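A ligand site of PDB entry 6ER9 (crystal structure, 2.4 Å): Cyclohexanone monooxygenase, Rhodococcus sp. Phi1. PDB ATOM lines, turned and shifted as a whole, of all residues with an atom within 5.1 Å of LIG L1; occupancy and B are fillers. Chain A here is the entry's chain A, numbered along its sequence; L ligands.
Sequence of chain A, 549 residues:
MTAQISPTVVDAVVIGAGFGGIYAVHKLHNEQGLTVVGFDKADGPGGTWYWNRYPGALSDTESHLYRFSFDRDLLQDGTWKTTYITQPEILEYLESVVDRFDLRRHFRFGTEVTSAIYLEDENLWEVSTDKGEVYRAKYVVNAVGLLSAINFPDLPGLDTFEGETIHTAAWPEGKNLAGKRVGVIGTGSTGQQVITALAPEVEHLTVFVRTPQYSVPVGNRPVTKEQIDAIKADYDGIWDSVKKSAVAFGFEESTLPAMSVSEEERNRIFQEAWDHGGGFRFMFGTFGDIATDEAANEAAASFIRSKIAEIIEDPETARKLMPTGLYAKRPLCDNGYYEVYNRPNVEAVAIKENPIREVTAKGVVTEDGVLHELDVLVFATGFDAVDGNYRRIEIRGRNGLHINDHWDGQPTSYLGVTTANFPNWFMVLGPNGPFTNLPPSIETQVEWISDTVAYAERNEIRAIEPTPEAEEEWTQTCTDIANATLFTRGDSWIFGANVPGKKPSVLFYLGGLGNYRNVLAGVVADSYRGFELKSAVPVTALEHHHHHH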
ATOM      1  N   TYR A  54       3.243 -13.383  -2.782  1.00  0.00           N
ATOM      2  CA  TYR A  54       4.326 -14.312  -3.044  1.00  0.00           C
ATOM      3  C   TYR A  54       4.866 -14.089  -4.459  1.00  0.00           C
ATOM      4  O   TYR A  54       4.140 -13.635  -5.346  1.00  0.00           O
ATOM      5  CB  TYR A  54       3.836 -15.751  -2.885  1.00  0.00           C
ATOM      6  CG  TYR A  54       2.745 -16.203  -3.833  1.00  0.00           C
ATOM      7  CD1 TYR A  54       3.070 -16.762  -5.069  1.00  0.00           C
ATOM      8  CD2 TYR A  54       1.393 -16.128  -3.494  1.00  0.00           C
ATOM      9  CE1 TYR A  54       2.106 -17.190  -5.943  1.00  0.00           C
ATOM     10  CE2 TYR A  54       0.404 -16.581  -4.388  1.00  0.00           C
ATOM     11  CZ  TYR A  54       0.774 -17.106  -5.615  1.00  0.00           C
ATOM     12  OH  TYR A  54      -0.144 -17.560  -6.536  1.00  0.00           O
ATOM     13  N   LEU A  58       0.059 -14.499 -10.171  1.00  0.00           N
ATOM     14  CA  LEU A  58      -0.456 -14.116 -11.475  1.00  0.00           C
ATOM     15  C   LEU A  58      -1.800 -14.778 -11.691  1.00  0.00           C
ATOM     16  O   LEU A  58      -2.060 -15.868 -11.160  1.00  0.00           O
ATOM     17  CB  LEU A  58       0.540 -14.504 -12.573  1.00  0.00           C
ATOM     18  CG  LEU A  58       0.266 -14.348 -14.075  1.00  0.00           C
ATOM     19  CD1 LEU A  58       1.403 -13.614 -14.782  1.00  0.00           C
ATOM     20  CD2 LEU A  58       0.054 -15.696 -14.739  1.00  0.00           C
ATOM     21  N   SER A  59      -2.674 -14.102 -12.442  1.00  0.00           N
ATOM     22  CA  SER A  59      -4.004 -14.601 -12.767  1.00  0.00           C
ATOM     23  C   SER A  59      -3.975 -15.455 -14.019  1.00  0.00           C
ATOM     24  O   SER A  59      -3.343 -15.088 -15.019  1.00  0.00           O
ATOM     25  CB  SER A  59      -4.940 -13.439 -13.042  1.00  0.00           C
ATOM     26  OG  SER A  59      -4.708 -12.976 -14.372  1.00  0.00           O
ATOM     27  N   ASP A  60      -4.723 -16.552 -13.995  1.00  0.00           N
ATOM     28  CA  ASP A  60      -4.990 -17.344 -15.201  1.00  0.00           C
ATOM     29  C   ASP A  60      -6.231 -16.883 -15.965  1.00  0.00           C
ATOM     30  O   ASP A  60      -6.672 -17.584 -16.886  1.00  0.00           O
ATOM     31  CB  ASP A  60      -5.119 -18.822 -14.836  1.00  0.00           C
ATOM     32  CG  ASP A  60      -3.813 -19.408 -14.346  1.00  0.00           C
ATOM     33  OD1 ASP A  60      -2.756 -18.796 -14.612  1.00  0.00           O
ATOM     34  OD2 ASP A  60      -3.856 -20.452 -13.660  1.00  0.00           O
ATOM     35  N   LEU A 147     -11.617 -18.313  -1.621  1.00  0.00           N
ATOM     36  CA  LEU A 147     -10.255 -18.837  -1.457  1.00  0.00           C
ATOM     37  C   LEU A 147      -9.500 -17.865  -0.554  1.00  0.00           C
ATOM     38  O   LEU A 147      -8.546 -17.205  -0.983  1.00  0.00           O
ATOM     39  CB  LEU A 147      -9.554 -19.029  -2.810  1.00  0.00           C
ATOM     40  CG  LEU A 147     -10.058 -20.144  -3.723  1.00  0.00           C
ATOM     41  CD1 LEU A 147      -9.671 -19.909  -5.177  1.00  0.00           C
ATOM     42  CD2 LEU A 147      -9.607 -21.518  -3.256  1.00  0.00           C
ATOM     43  N   ASN A 151      -5.349 -22.283   4.893  1.00  0.00           N
ATOM     44  CA  ASN A 151      -5.120 -23.663   5.311  1.00  0.00           C
ATOM     45  C   ASN A 151      -3.638 -23.854   5.603  1.00  0.00           C
ATOM     46  O   ASN A 151      -2.799 -23.734   4.697  1.00  0.00           O
ATOM     47  CB  ASN A 151      -5.619 -24.645   4.255  1.00  0.00           C
ATOM     48  CG  ASN A 151      -5.274 -26.090   4.593  1.00  0.00           C
ATOM     49  OD1 ASN A 151      -4.570 -26.767   3.854  1.00  0.00           O
ATOM     50  ND2 ASN A 151      -5.791 -26.581   5.714  1.00  0.00           N
ATOM     51  N   PRO A 153      -1.362 -26.638   7.386  1.00  0.00           N
ATOM     52  CA  PRO A 153      -1.144 -27.921   8.071  1.00  0.00           C
ATOM     53  C   PRO A 153      -0.032 -27.858   9.115  1.00  0.00           C
ATOM     54  O   PRO A 153       0.934 -27.106   8.980  1.00  0.00           O
ATOM     55  CB  PRO A 153      -0.783 -28.873   6.918  1.00  0.00           C
ATOM     56  CG  PRO A 153      -1.413 -28.251   5.703  1.00  0.00           C
ATOM     57  CD  PRO A 153      -1.288 -26.768   5.918  1.00  0.00           C
ATOM     58  N   ILE A 185       6.602 -26.531   0.299  1.00  0.00           N
ATOM     59  CA  ILE A 185       5.650 -27.641   0.388  1.00  0.00           C
ATOM     60  C   ILE A 185       4.358 -27.208  -0.255  1.00  0.00           C
ATOM     61  O   ILE A 185       3.730 -26.233   0.171  1.00  0.00           O
ATOM     62  CB  ILE A 185       5.408 -28.070   1.835  1.00  0.00           C
ATOM     63  CG1 ILE A 185       6.741 -28.405   2.479  1.00  0.00           C
ATOM     64  CG2 ILE A 185       4.434 -29.234   1.870  1.00  0.00           C
ATOM     65  CD1 ILE A 185       6.679 -28.304   3.954  1.00  0.00           C
ATOM     66  N   GLY A 186       3.942 -27.944  -1.276  1.00  0.00           N
ATOM     67  CA  GLY A 186       2.752 -27.575  -2.015  1.00  0.00           C
ATOM     68  C   GLY A 186       2.994 -27.507  -3.506  1.00  0.00           C
ATOM     69  O   GLY A 186       3.917 -26.838  -3.974  1.00  0.00           O
ATOM     70  N   THR A 187       2.103 -28.156  -4.260  1.00  0.00           N
ATOM     71  CA  THR A 187       2.289 -28.359  -5.686  1.00  0.00           C
ATOM     72  C   THR A 187       1.013 -27.996  -6.475  1.00  0.00           C
ATOM     73  O   THR A 187       0.898 -28.304  -7.670  1.00  0.00           O
ATOM     74  CB  THR A 187       2.776 -29.814  -5.893  1.00  0.00           C
ATOM     75  OG1 THR A 187       4.179 -29.859  -5.598  1.00  0.00           O
ATOM     76  CG2 THR A 187       2.580 -30.352  -7.250  1.00  0.00           C
ATOM     77  N   GLY A 188       0.086 -27.277  -5.849  1.00  0.00           N
ATOM     78  CA  GLY A 188      -1.055 -26.762  -6.561  1.00  0.00           C
ATOM     79  C   GLY A 188      -0.620 -25.544  -7.349  1.00  0.00           C
ATOM     80  O   GLY A 188       0.580 -25.324  -7.565  1.00  0.00           O
ATOM     81  N   SER A 189      -1.597 -24.723  -7.752  1.00  0.00           N
ATOM     82  CA  SER A 189      -1.344 -23.531  -8.553  1.00  0.00           C
ATOM     83  C   SER A 189      -0.369 -22.567  -7.877  1.00  0.00           C
ATOM     84  O   SER A 189       0.424 -21.910  -8.551  1.00  0.00           O
ATOM     85  CB  SER A 189      -2.666 -22.823  -8.835  1.00  0.00           C
ATOM     86  OG  SER A 189      -2.553 -21.954  -9.944  1.00  0.00           O
ATOM     87  N   THR A 190      -0.462 -22.418  -6.545  1.00  0.00           N
ATOM     88  CA  THR A 190       0.385 -21.460  -5.858  1.00  0.00           C
ATOM     89  C   THR A 190       1.813 -21.956  -5.798  1.00  0.00           C
ATOM     90  O   THR A 190       2.763 -21.219  -6.116  1.00  0.00           O
ATOM     91  CB  THR A 190      -0.114 -21.179  -4.442  1.00  0.00           C
ATOM     92  OG1 THR A 190      -1.412 -20.551  -4.486  1.00  0.00           O
ATOM     93  CG2 THR A 190       0.885 -20.311  -3.694  1.00  0.00           C
ATOM     94  N   GLY A 191       1.993 -23.213  -5.365  1.00  0.00           N
ATOM     95  CA  GLY A 191       3.307 -23.811  -5.357  1.00  0.00           C
ATOM     96  C   GLY A 191       4.009 -23.737  -6.698  1.00  0.00           C
ATOM     97  O   GLY A 191       5.176 -23.386  -6.775  1.00  0.00           O
ATOM     98  N   GLN A 193       3.630 -21.563  -9.149  1.00  0.00           N
ATOM     99  CA  GLN A 193       4.064 -20.187  -9.415  1.00  0.00           C
ATOM    100  C   GLN A 193       5.278 -19.806  -8.582  1.00  0.00           C
ATOM    101  O   GLN A 193       6.241 -19.207  -9.092  1.00  0.00           O
ATOM    102  CB  GLN A 193       2.909 -19.205  -9.159  1.00  0.00           C
ATOM    103  CG  GLN A 193       1.777 -19.320 -10.163  1.00  0.00           C
ATOM    104  CD  GLN A 193       0.740 -18.199 -10.031  1.00  0.00           C
ATOM    105  OE1 GLN A 193       0.548 -17.633  -8.940  1.00  0.00           O
ATOM    106  NE2 GLN A 193       0.082 -17.878 -11.140  1.00  0.00           N
ATOM    107  N   ARG A 210       3.929 -33.977  -2.822  1.00  0.00           N
ATOM    108  CA  ARG A 210       3.067 -35.080  -2.384  1.00  0.00           C
ATOM    109  C   ARG A 210       2.183 -35.587  -3.513  1.00  0.00           C
ATOM    110  O   ARG A 210       2.136 -36.796  -3.770  1.00  0.00           O
ATOM    111  CB  ARG A 210       2.194 -34.637  -1.195  1.00  0.00           C
ATOM    112  CG  ARG A 210       1.443 -35.773  -0.498  1.00  0.00           C
ATOM    113  CD  ARG A 210       0.778 -35.319   0.800  1.00  0.00           C
ATOM    114  NE  ARG A 210      -0.434 -34.534   0.543  1.00  0.00           N
ATOM    115  CZ  ARG A 210      -1.171 -33.942   1.486  1.00  0.00           C
ATOM    116  NH1 ARG A 210      -0.832 -34.039   2.766  1.00  0.00           N
ATOM    117  NH2 ARG A 210      -2.247 -33.252   1.149  1.00  0.00           N
ATOM    118  N   THR A 211       1.503 -34.687  -4.220  1.00  0.00           N
ATOM    119  CA  THR A 211       0.682 -35.056  -5.366  1.00  0.00           C
ATOM    120  C   THR A 211       1.072 -34.178  -6.550  1.00  0.00           C
ATOM    121  O   THR A 211       0.675 -33.005  -6.601  1.00  0.00           O
ATOM    122  CB  THR A 211      -0.799 -34.895  -5.061  1.00  0.00           C
ATOM    123  OG1 THR A 211      -1.124 -35.687  -3.907  1.00  0.00           O
ATOM    124  CG2 THR A 211      -1.629 -35.349  -6.236  1.00  0.00           C
ATOM    125  N   GLN A 213       0.719 -32.611 -10.208  1.00  0.00           N
ATOM    126  CA  GLN A 213      -0.488 -32.223 -10.926  1.00  0.00           C
ATOM    127  C   GLN A 213      -0.205 -32.011 -12.414  1.00  0.00           C
ATOM    128  O   GLN A 213       0.951 -31.988 -12.852  1.00  0.00           O
ATOM    129  CB  GLN A 213      -1.064 -30.932 -10.337  1.00  0.00           C
ATOM    130  CG  GLN A 213      -1.570 -31.099  -8.931  1.00  0.00           C
ATOM    131  CD  GLN A 213      -2.747 -30.209  -8.671  1.00  0.00           C
ATOM    132  OE1 GLN A 213      -3.610 -30.058  -9.529  1.00  0.00           O
ATOM    133  NE2 GLN A 213      -2.767 -29.592  -7.492  1.00  0.00           N
ATOM    134  N   LYS A 329      -8.843 -31.729 -11.542  1.00  0.00           N
ATOM    135  CA  LYS A 329      -8.625 -30.617 -10.629  1.00  0.00           C
ATOM    136  C   LYS A 329      -8.662 -29.316 -11.406  1.00  0.00           C
ATOM    137  O   LYS A 329      -8.677 -29.313 -12.645  1.00  0.00           O
ATOM    138  CB  LYS A 329      -7.279 -30.756  -9.890  1.00  0.00           C
ATOM    139  CG  LYS A 329      -7.202 -31.883  -8.888  1.00  0.00           C
ATOM    140  CD  LYS A 329      -5.788 -31.971  -8.319  1.00  0.00           C
ATOM    141  CE  LYS A 329      -5.775 -32.568  -6.933  1.00  0.00           C
ATOM    142  NZ  LYS A 329      -5.654 -34.045  -6.947  1.00  0.00           N
ATOM    143  N   ARG A 330      -8.670 -28.197 -10.675  1.00  0.00           N
ATOM    144  CA  ARG A 330      -8.720 -26.883 -11.286  1.00  0.00           C
ATOM    145  C   ARG A 330      -7.585 -26.750 -12.291  1.00  0.00           C
ATOM    146  O   ARG A 330      -6.408 -26.857 -11.908  1.00  0.00           O
ATOM    147  CB  ARG A 330      -8.606 -25.780 -10.241  1.00  0.00           C
ATOM    148  CG  ARG A 330      -8.889 -24.386 -10.771  1.00  0.00           C
ATOM    149  CD  ARG A 330      -7.595 -23.652 -11.145  1.00  0.00           C
ATOM    150  NE  ARG A 330      -7.825 -22.253 -11.478  1.00  0.00           N
ATOM    151  CZ  ARG A 330      -6.907 -21.426 -11.967  1.00  0.00           C
ATOM    152  NH1 ARG A 330      -5.668 -21.847 -12.192  1.00  0.00           N
ATOM    153  NH2 ARG A 330      -7.228 -20.168 -12.236  1.00  0.00           N
ATOM    154  N   LYS A 352       5.144 -38.932  -0.502  1.00  0.00           N
ATOM    155  CA  LYS A 352       4.360 -40.142  -0.284  1.00  0.00           C
ATOM    156  C   LYS A 352       5.242 -41.379  -0.141  1.00  0.00           C
ATOM    157  O   LYS A 352       4.875 -42.315   0.577  1.00  0.00           O
ATOM    158  CB  LYS A 352       3.351 -40.318  -1.408  1.00  0.00           C
ATOM    159  CG  LYS A 352       1.937 -39.937  -1.001  1.00  0.00           C
ATOM    160  CD  LYS A 352       1.033 -39.707  -2.207  1.00  0.00           C
ATOM    161  CE  LYS A 352      -0.314 -39.159  -1.759  1.00  0.00           C
ATOM    162  NZ  LYS A 352      -1.247 -38.874  -2.891  1.00  0.00           N
ATOM    163  N   ALA A 380       2.984 -23.673   0.644  1.00  0.00           N
ATOM    164  CA  ALA A 380       2.072 -23.422  -0.471  1.00  0.00           C
ATOM    165  C   ALA A 380       0.829 -24.282  -0.370  1.00  0.00           C
ATOM    166  O   ALA A 380       0.401 -24.897  -1.349  1.00  0.00           O
ATOM    167  CB  ALA A 380       2.800 -23.645  -1.783  1.00  0.00           C
ATOM    168  N   THR A 381       0.236 -24.338   0.810  1.00  0.00           N
ATOM    169  CA  THR A 381      -0.930 -25.172   1.052  1.00  0.00           C
ATOM    170  C   THR A 381      -2.195 -24.378   0.716  1.00  0.00           C
ATOM    171  O   THR A 381      -2.131 -23.210   0.340  1.00  0.00           O
ATOM    172  CB  THR A 381      -0.912 -25.700   2.483  1.00  0.00           C
ATOM    173  OG1 THR A 381      -0.628 -24.645   3.397  1.00  0.00           O
ATOM    174  CG2 THR A 381       0.198 -26.757   2.615  1.00  0.00           C
ATOM    175  N   GLY A 382      -3.333 -25.039   0.796  1.00  0.00           N
ATOM    176  CA  GLY A 382      -4.542 -24.491   0.197  1.00  0.00           C
ATOM    177  C   GLY A 382      -5.324 -23.535   1.070  1.00  0.00           C
ATOM    178  O   GLY A 382      -4.782 -22.763   1.869  1.00  0.00           O
ATOM    179  N   PHE A 383      -6.649 -23.600   0.912  1.00  0.00           N
ATOM    180  CA  PHE A 383      -7.577 -22.776   1.660  1.00  0.00           C
ATOM    181  C   PHE A 383      -8.700 -23.666   2.183  1.00  0.00           C
ATOM    182  O   PHE A 383      -9.083 -24.653   1.554  1.00  0.00           O
ATOM    183  CB  PHE A 383      -8.181 -21.652   0.786  1.00  0.00           C
ATOM    184  CG  PHE A 383      -7.148 -20.751   0.157  1.00  0.00           C
ATOM    185  CD1 PHE A 383      -6.599 -21.051  -1.089  1.00  0.00           C
ATOM    186  CD2 PHE A 383      -6.728 -19.589   0.806  1.00  0.00           C
ATOM    187  CE1 PHE A 383      -5.647 -20.217  -1.667  1.00  0.00           C
ATOM    188  CE2 PHE A 383      -5.776 -18.755   0.229  1.00  0.00           C
ATOM    189  CZ  PHE A 383      -5.245 -19.080  -1.015  1.00  0.00           C
ATOM    190  N   TRP A 493      -9.838 -29.246  -3.297  1.00  0.00           N
ATOM    191  CA  TRP A 493     -10.589 -28.310  -2.474  1.00  0.00           C
ATOM    192  C   TRP A 493     -11.962 -27.989  -3.067  1.00  0.00           C
ATOM    193  O   TRP A 493     -12.829 -27.507  -2.346  1.00  0.00           O
ATOM    194  CB  TRP A 493      -9.800 -27.004  -2.298  1.00  0.00           C
ATOM    195  CG  TRP A 493      -9.602 -26.241  -3.603  1.00  0.00           C
ATOM    196  CD1 TRP A 493      -8.523 -26.316  -4.439  1.00  0.00           C
ATOM    197  CD2 TRP A 493     -10.509 -25.297  -4.211  1.00  0.00           C
ATOM    198  NE1 TRP A 493      -8.697 -25.484  -5.524  1.00  0.00           N
ATOM    199  CE2 TRP A 493      -9.907 -24.852  -5.408  1.00  0.00           C
ATOM    200  CE3 TRP A 493     -11.765 -24.794  -3.862  1.00  0.00           C
ATOM    201  CZ2 TRP A 493     -10.516 -23.915  -6.247  1.00  0.00           C
ATOM    202  CZ3 TRP A 493     -12.374 -23.857  -4.701  1.00  0.00           C
ATOM    203  CH2 TRP A 493     -11.747 -23.432  -5.879  1.00  0.00           C
ATOM    204  N   ASN A 498      -9.737 -31.233   0.945  1.00  0.00           N
ATOM    205  CA  ASN A 498      -8.359 -30.861   1.224  1.00  0.00           C
ATOM    206  C   ASN A 498      -8.103 -30.507   2.690  1.00  0.00           C
ATOM    207  O   ASN A 498      -6.941 -30.427   3.091  1.00  0.00           O
ATOM    208  CB  ASN A 498      -7.941 -29.683   0.338  1.00  0.00           C
ATOM    209  CG  ASN A 498      -8.779 -28.442   0.597  1.00  0.00           C
ATOM    210  OD1 ASN A 498     -10.006 -28.510   0.675  1.00  0.00           O
ATOM    211  ND2 ASN A 498      -8.122 -27.296   0.748  1.00  0.00           N
HETATM  212  P1  LIG L   1      -4.236 -26.124  -3.330  1.00  0.00           P
HETATM  213  O1  LIG L   1      -4.755 -26.390  -4.689  1.00  0.00           O
HETATM  214  O2  LIG L   1      -5.148 -26.663  -2.240  1.00  0.00           O
HETATM  215  O3  LIG L   1      -2.748 -26.715  -3.095  1.00  0.00           O
HETATM  216  C1  LIG L   1      -2.297 -27.105  -1.783  1.00  0.00           C
HETATM  217  C2  LIG L   1      -1.021 -27.893  -1.961  1.00  0.00           C
HETATM  218  O4  LIG L   1      -0.467 -28.205  -0.665  1.00  0.00           O
HETATM  219  C3  LIG L   1      -1.191 -29.232  -2.690  1.00  0.00           C
HETATM  220  O5  LIG L   1      -0.056 -29.526  -3.486  1.00  0.00           O
HETATM  221  C4  LIG L   1      -1.322 -30.210  -1.521  1.00  0.00           C
HETATM  222  O6  LIG L   1      -1.058 -31.581  -1.870  1.00  0.00           O
HETATM  223  C5  LIG L   1      -0.341 -29.606  -0.527  1.00  0.00           C
HETATM  224  N1  LIG L   1      -0.632 -29.955   0.870  1.00  0.00           N
HETATM  225  C6  LIG L   1      -1.795 -29.726   1.546  1.00  0.00           C
HETATM  226  N2  LIG L   1      -1.764 -30.141   2.790  1.00  0.00           N
HETATM  227  C7  LIG L   1      -0.513 -30.689   2.943  1.00  0.00           C
HETATM  228  C8  LIG L   1       0.133 -31.336   4.013  1.00  0.00           C
HETATM  229  N3  LIG L   1      -0.452 -31.577   5.182  1.00  0.00           N
HETATM  230  N4  LIG L   1       1.395 -31.772   3.821  1.00  0.00           N
HETATM  231  C9  LIG L   1       1.956 -31.608   2.617  1.00  0.00           C
HETATM  232  N5  LIG L   1       1.450 -31.028   1.525  1.00  0.00           N
HETATM  233  C10 LIG L   1       0.215 -30.585   1.747  1.00  0.00           C
HETATM  234  O7  LIG L   1      -4.018 -24.562  -3.124  1.00  0.00           O
HETATM  235  P2  LIG L   1      -3.227 -23.467  -3.964  1.00  0.00           P
HETATM  236  O8  LIG L   1      -2.207 -24.114  -4.817  1.00  0.00           O
HETATM  237  O9  LIG L   1      -2.793 -22.406  -3.021  1.00  0.00           O
HETATM  238  O10 LIG L   1      -4.385 -22.963  -4.940  1.00  0.00           O
HETATM  239  C11 LIG L   1      -5.775 -23.140  -4.552  1.00  0.00           C
HETATM  240  C12 LIG L   1      -6.675 -22.513  -5.596  1.00  0.00           C
HETATM  241  O11 LIG L   1      -6.447 -21.081  -5.634  1.00  0.00           O
HETATM  242  C13 LIG L   1      -6.462 -22.977  -7.035  1.00  0.00           C
HETATM  243  O12 LIG L   1      -7.108 -24.210  -7.364  1.00  0.00           O
HETATM  244  C14 LIG L   1      -7.052 -21.795  -7.819  1.00  0.00           C
HETATM  245  O13 LIG L   1      -8.476 -21.807  -7.859  1.00  0.00           O
HETATM  246  C15 LIG L   1      -6.573 -20.624  -6.966  1.00  0.00           C
HETATM  247  N6  LIG L   1      -5.222 -20.078  -7.419  1.00  0.00           N
HETATM  248  C16 LIG L   1      -5.217 -19.620  -8.681  1.00  0.00           C
HETATM  249  C17 LIG L   1      -4.039 -19.174  -9.252  1.00  0.00           C
HETATM  250  C18 LIG L   1      -4.066 -18.622 -10.656  1.00  0.00           C
HETATM  251  O14 LIG L   1      -2.990 -18.388 -11.233  1.00  0.00           O
HETATM  252  N7  LIG L   1      -5.243 -18.494 -11.247  1.00  0.00           N
HETATM  253  C19 LIG L   1      -2.882 -19.196  -8.487  1.00  0.00           C
HETATM  254  C20 LIG L   1      -2.913 -19.664  -7.190  1.00  0.00           C
HETATM  255  C21 LIG L   1      -4.101 -20.100  -6.663  1.00  0.00           C
HETATM  256  P3  LIG L   1      -2.259 -32.654  -2.167  1.00  0.00           P
HETATM  257  O15 LIG L   1      -2.895 -32.456  -3.507  1.00  0.00           O
HETATM  258  O16 LIG L   1      -1.558 -34.021  -2.019  1.00  0.00           O
HETATM  259  O17 LIG L   1      -3.275 -32.583  -1.042  1.00  0.00           O
HETATM  260  P1  LG2 L   2     -11.324 -12.011  -1.630  1.00  0.00           P
HETATM  261  O1  LG2 L   2     -10.439 -11.340  -2.604  1.00  0.00           O
HETATM  262  O2  LG2 L   2     -10.751 -13.277  -0.964  1.00  0.00           O
HETATM  263  O3  LG2 L   2     -11.657 -10.923  -0.486  1.00  0.00           O
HETATM  264  C1  LG2 L   2     -12.186 -11.411   0.759  1.00  0.00           C
HETATM  265  C2  LG2 L   2     -11.760 -10.422   1.807  1.00  0.00           C
HETATM  266  O4  LG2 L   2     -12.599 -10.555   2.963  1.00  0.00           O
HETATM  267  C3  LG2 L   2     -10.308 -10.582   2.287  1.00  0.00           C
HETATM  268  O5  LG2 L   2      -9.535  -9.389   2.107  1.00  0.00           O
HETATM  269  C4  LG2 L   2     -10.441 -10.923   3.784  1.00  0.00           C
HETATM  270  O6  LG2 L   2      -9.406 -10.239   4.490  1.00  0.00           O
HETATM  271  C5  LG2 L   2     -11.815 -10.316   4.107  1.00  0.00           C
HETATM  272  N1  LG2 L   2     -12.487 -10.905   5.267  1.00  0.00           N
HETATM  273  C6  LG2 L   2     -12.908 -12.194   5.428  1.00  0.00           C
HETATM  274  N2  LG2 L   2     -13.463 -12.446   6.588  1.00  0.00           N
HETATM  275  C7  LG2 L   2     -13.404 -11.220   7.240  1.00  0.00           C
HETATM  276  C8  LG2 L   2     -13.836 -10.794   8.518  1.00  0.00           C
HETATM  277  N3  LG2 L   2     -14.377 -11.605   9.432  1.00  0.00           N
HETATM  278  N4  LG2 L   2     -13.674  -9.492   8.832  1.00  0.00           N
HETATM  279  C9  LG2 L   2     -13.081  -8.690   7.949  1.00  0.00           C
HETATM  280  N5  LG2 L   2     -12.606  -8.974   6.738  1.00  0.00           N
HETATM  281  C10 LG2 L   2     -12.805 -10.263   6.440  1.00  0.00           C
HETATM  282  N6  LG2 L   2     -10.048 -16.127  -9.985  1.00  0.00           N
HETATM  283  C11 LG2 L   2     -10.225 -16.017 -11.317  1.00  0.00           C
HETATM  284  O7  LG2 L   2     -11.367 -15.964 -11.798  1.00  0.00           O
HETATM  285  N7  LG2 L   2      -9.131 -15.968 -12.158  1.00  0.00           N
HETATM  286  C12 LG2 L   2      -7.801 -15.999 -11.764  1.00  0.00           C
HETATM  287  O8  LG2 L   2      -6.917 -15.891 -12.598  1.00  0.00           O
HETATM  288  C13 LG2 L   2      -7.619 -16.124 -10.329  1.00  0.00           C
HETATM  289  N8  LG2 L   2      -6.401 -16.212  -9.875  1.00  0.00           N
HETATM  290  C14 LG2 L   2      -6.236 -16.369  -8.497  1.00  0.00           C
HETATM  291  C15 LG2 L   2      -4.938 -16.413  -7.980  1.00  0.00           C
HETATM  292  C16 LG2 L   2      -4.717 -16.567  -6.616  1.00  0.00           C
HETATM  293  C17 LG2 L   2      -3.318 -16.478  -6.072  1.00  0.00           C
HETATM  294  C18 LG2 L   2      -5.816 -16.718  -5.750  1.00  0.00           C
HETATM  295  C19 LG2 L   2      -5.615 -16.956  -4.275  1.00  0.00           C
HETATM  296  C20 LG2 L   2      -7.109 -16.662  -6.265  1.00  0.00           C
HETATM  297  C21 LG2 L   2      -7.323 -16.463  -7.634  1.00  0.00           C
HETATM  298  N9  LG2 L   2      -8.629 -16.330  -8.171  1.00  0.00           N
HETATM  299  C22 LG2 L   2      -8.814 -16.176  -9.525  1.00  0.00           C
HETATM  300  C23 LG2 L   2      -9.883 -16.330  -7.404  1.00  0.00           C
HETATM  301  C24 LG2 L   2     -10.812 -15.118  -7.238  1.00  0.00           C
HETATM  302  O9  LG2 L   2     -10.921 -14.301  -8.399  1.00  0.00           O
HETATM  303  C25 LG2 L   2     -10.272 -14.211  -6.143  1.00  0.00           C
HETATM  304  O10 LG2 L   2     -10.174 -15.045  -4.991  1.00  0.00           O
HETATM  305  C26 LG2 L   2     -11.187 -12.994  -5.995  1.00  0.00           C
HETATM  306  O11 LG2 L   2     -10.388 -11.808  -5.926  1.00  0.00           O
HETATM  307  C27 LG2 L   2     -12.240 -13.094  -4.907  1.00  0.00           C
HETATM  308  O12 LG2 L   2     -12.753 -11.786  -4.622  1.00  0.00           O
HETATM  309  P2  LG2 L   2     -13.655 -11.645  -3.327  1.00  0.00           P
HETATM  310  O13 LG2 L   2     -13.897 -10.199  -3.131  1.00  0.00           O
HETATM  311  O14 LG2 L   2     -14.958 -12.464  -3.463  1.00  0.00           O
HETATM  312  O15 LG2 L   2     -12.788 -12.322  -2.165  1.00  0.00           O
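NH2 of Arg 210 lies within salt-bridge range of O17 of LIG L1 (2.5 Å). The side-chain hydroxyl (OG1) of Thr 211 is in hydrogen-bond range of an oxygen (O16) of LIG L1 (2.6 Å). The backbone NH of Thr 187 lies within hydrogen-bond range of an oxygen (O5) of LIG L1, 2.7 Å away. The backbone carbonyl oxygen of Leu 58 lies close to an oxygen (O14) of LIG L1 (2.7 Å). The backbone NH (N) of Thr 190 is in hydrogen-bond range of an oxygen (O8) of LIG L1 (3.0 Å). An oxygen (O9) of LIG L1 sits at hydrogen-bond distance from the side-chain hydroxyl (OG1) of Thr 190. The indole nitrogen (NE1) of Trp 493 lies within hydrogen-bond range of an oxygen (O12) of LIG L1, 2.7 Å away. The backbone NH (N) of Ser 189 sits at hydrogen-bond distance from an oxygen (O8) of LIG L1, 3.1 Å away. An oxygen (O14) of LIG L1 sits at hydrogen-bond distance from the side-chain amide nitrogen (NE2) of Gln 193 (3.1 Å). The backbone NH of Gly 188 sits at hydrogen-bond distance from an oxygen (O5) of LIG L1. A nitrogen (N7) of LIG L1 lies within hydrogen-bond range of the side-chain carboxylate (OD2) of Asp 60 (3.4 Å). An oxygen (O8) of LG2 L2 sits at hydrogen-bond distance from the backbone NH of Asp 60, at 2.7 Å.
N7 of LIG L1 sits at hydrogen-bond distance from N8 of LG2 L2 (2.9 Å).
The side-chain amino group (NZ) of Lys 352 lies within hydrogen-bond range of the side-chain hydroxyl (OG1) of Thr 211 (3.3 Å). NE2 of Gln 193 is in hydrogen-bond range of O of Leu 58 (2.9 Å). NH1 of Arg 330 is in salt-bridge range of OD2 of Asp 60, at 2.7 Å. The side-chain amide oxygen (OE1) of Gln 193 is in hydrogen-bond range of the side-chain hydroxyl (OH) of Tyr 54 (2.5 Å). O of Gly 382 lies within hydrogen-bond range of N of Asn 151. O of Ile 185 is in hydrogen-bond range of N of Ala 380, 2.7 Å away. OG1 of Thr 381 sits at hydrogen-bond distance from O of Asn 151 (2.7 Å). O of Phe 383 is in hydrogen-bond range of ND2 of Asn 498, at 2.9 Å.
NH2 of Arg 330 sits close to N7 of LIG L1. The backbone carbonyl oxygen (O) of Ala 380 lies close to an oxygen (O4) of LIG L1 (3.5 Å). Residues that only touch LIG L1: Tyr 54 (3.5 Å), Leu 147 (3.5 Å), Pro 153 (3.2 Å), Ile 185 (3.5 Å), Gly 186 (3.5 Å), Thr 381 (3.5 Å), Gly 382 (3.3 Å) and Phe 383 (3.8 Å). Hydrophobic or aromatic side chains that line LIG L1: Leu 147, Pro 153, Ile 185, Phe 383 and Trp 493. 20 residues have an atom within 4 Å of LIG L1: Tyr 54, Leu 58, Asp 60, Leu 147, Pro 153, Ile 185, Gly 186, Thr 187, Gly 188, Ser 189, Thr 190, Gln 193, Arg 210, Thr 211, Arg 330, Ala 380, Thr 381, Gly 382, Phe 383 and Trp 493.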
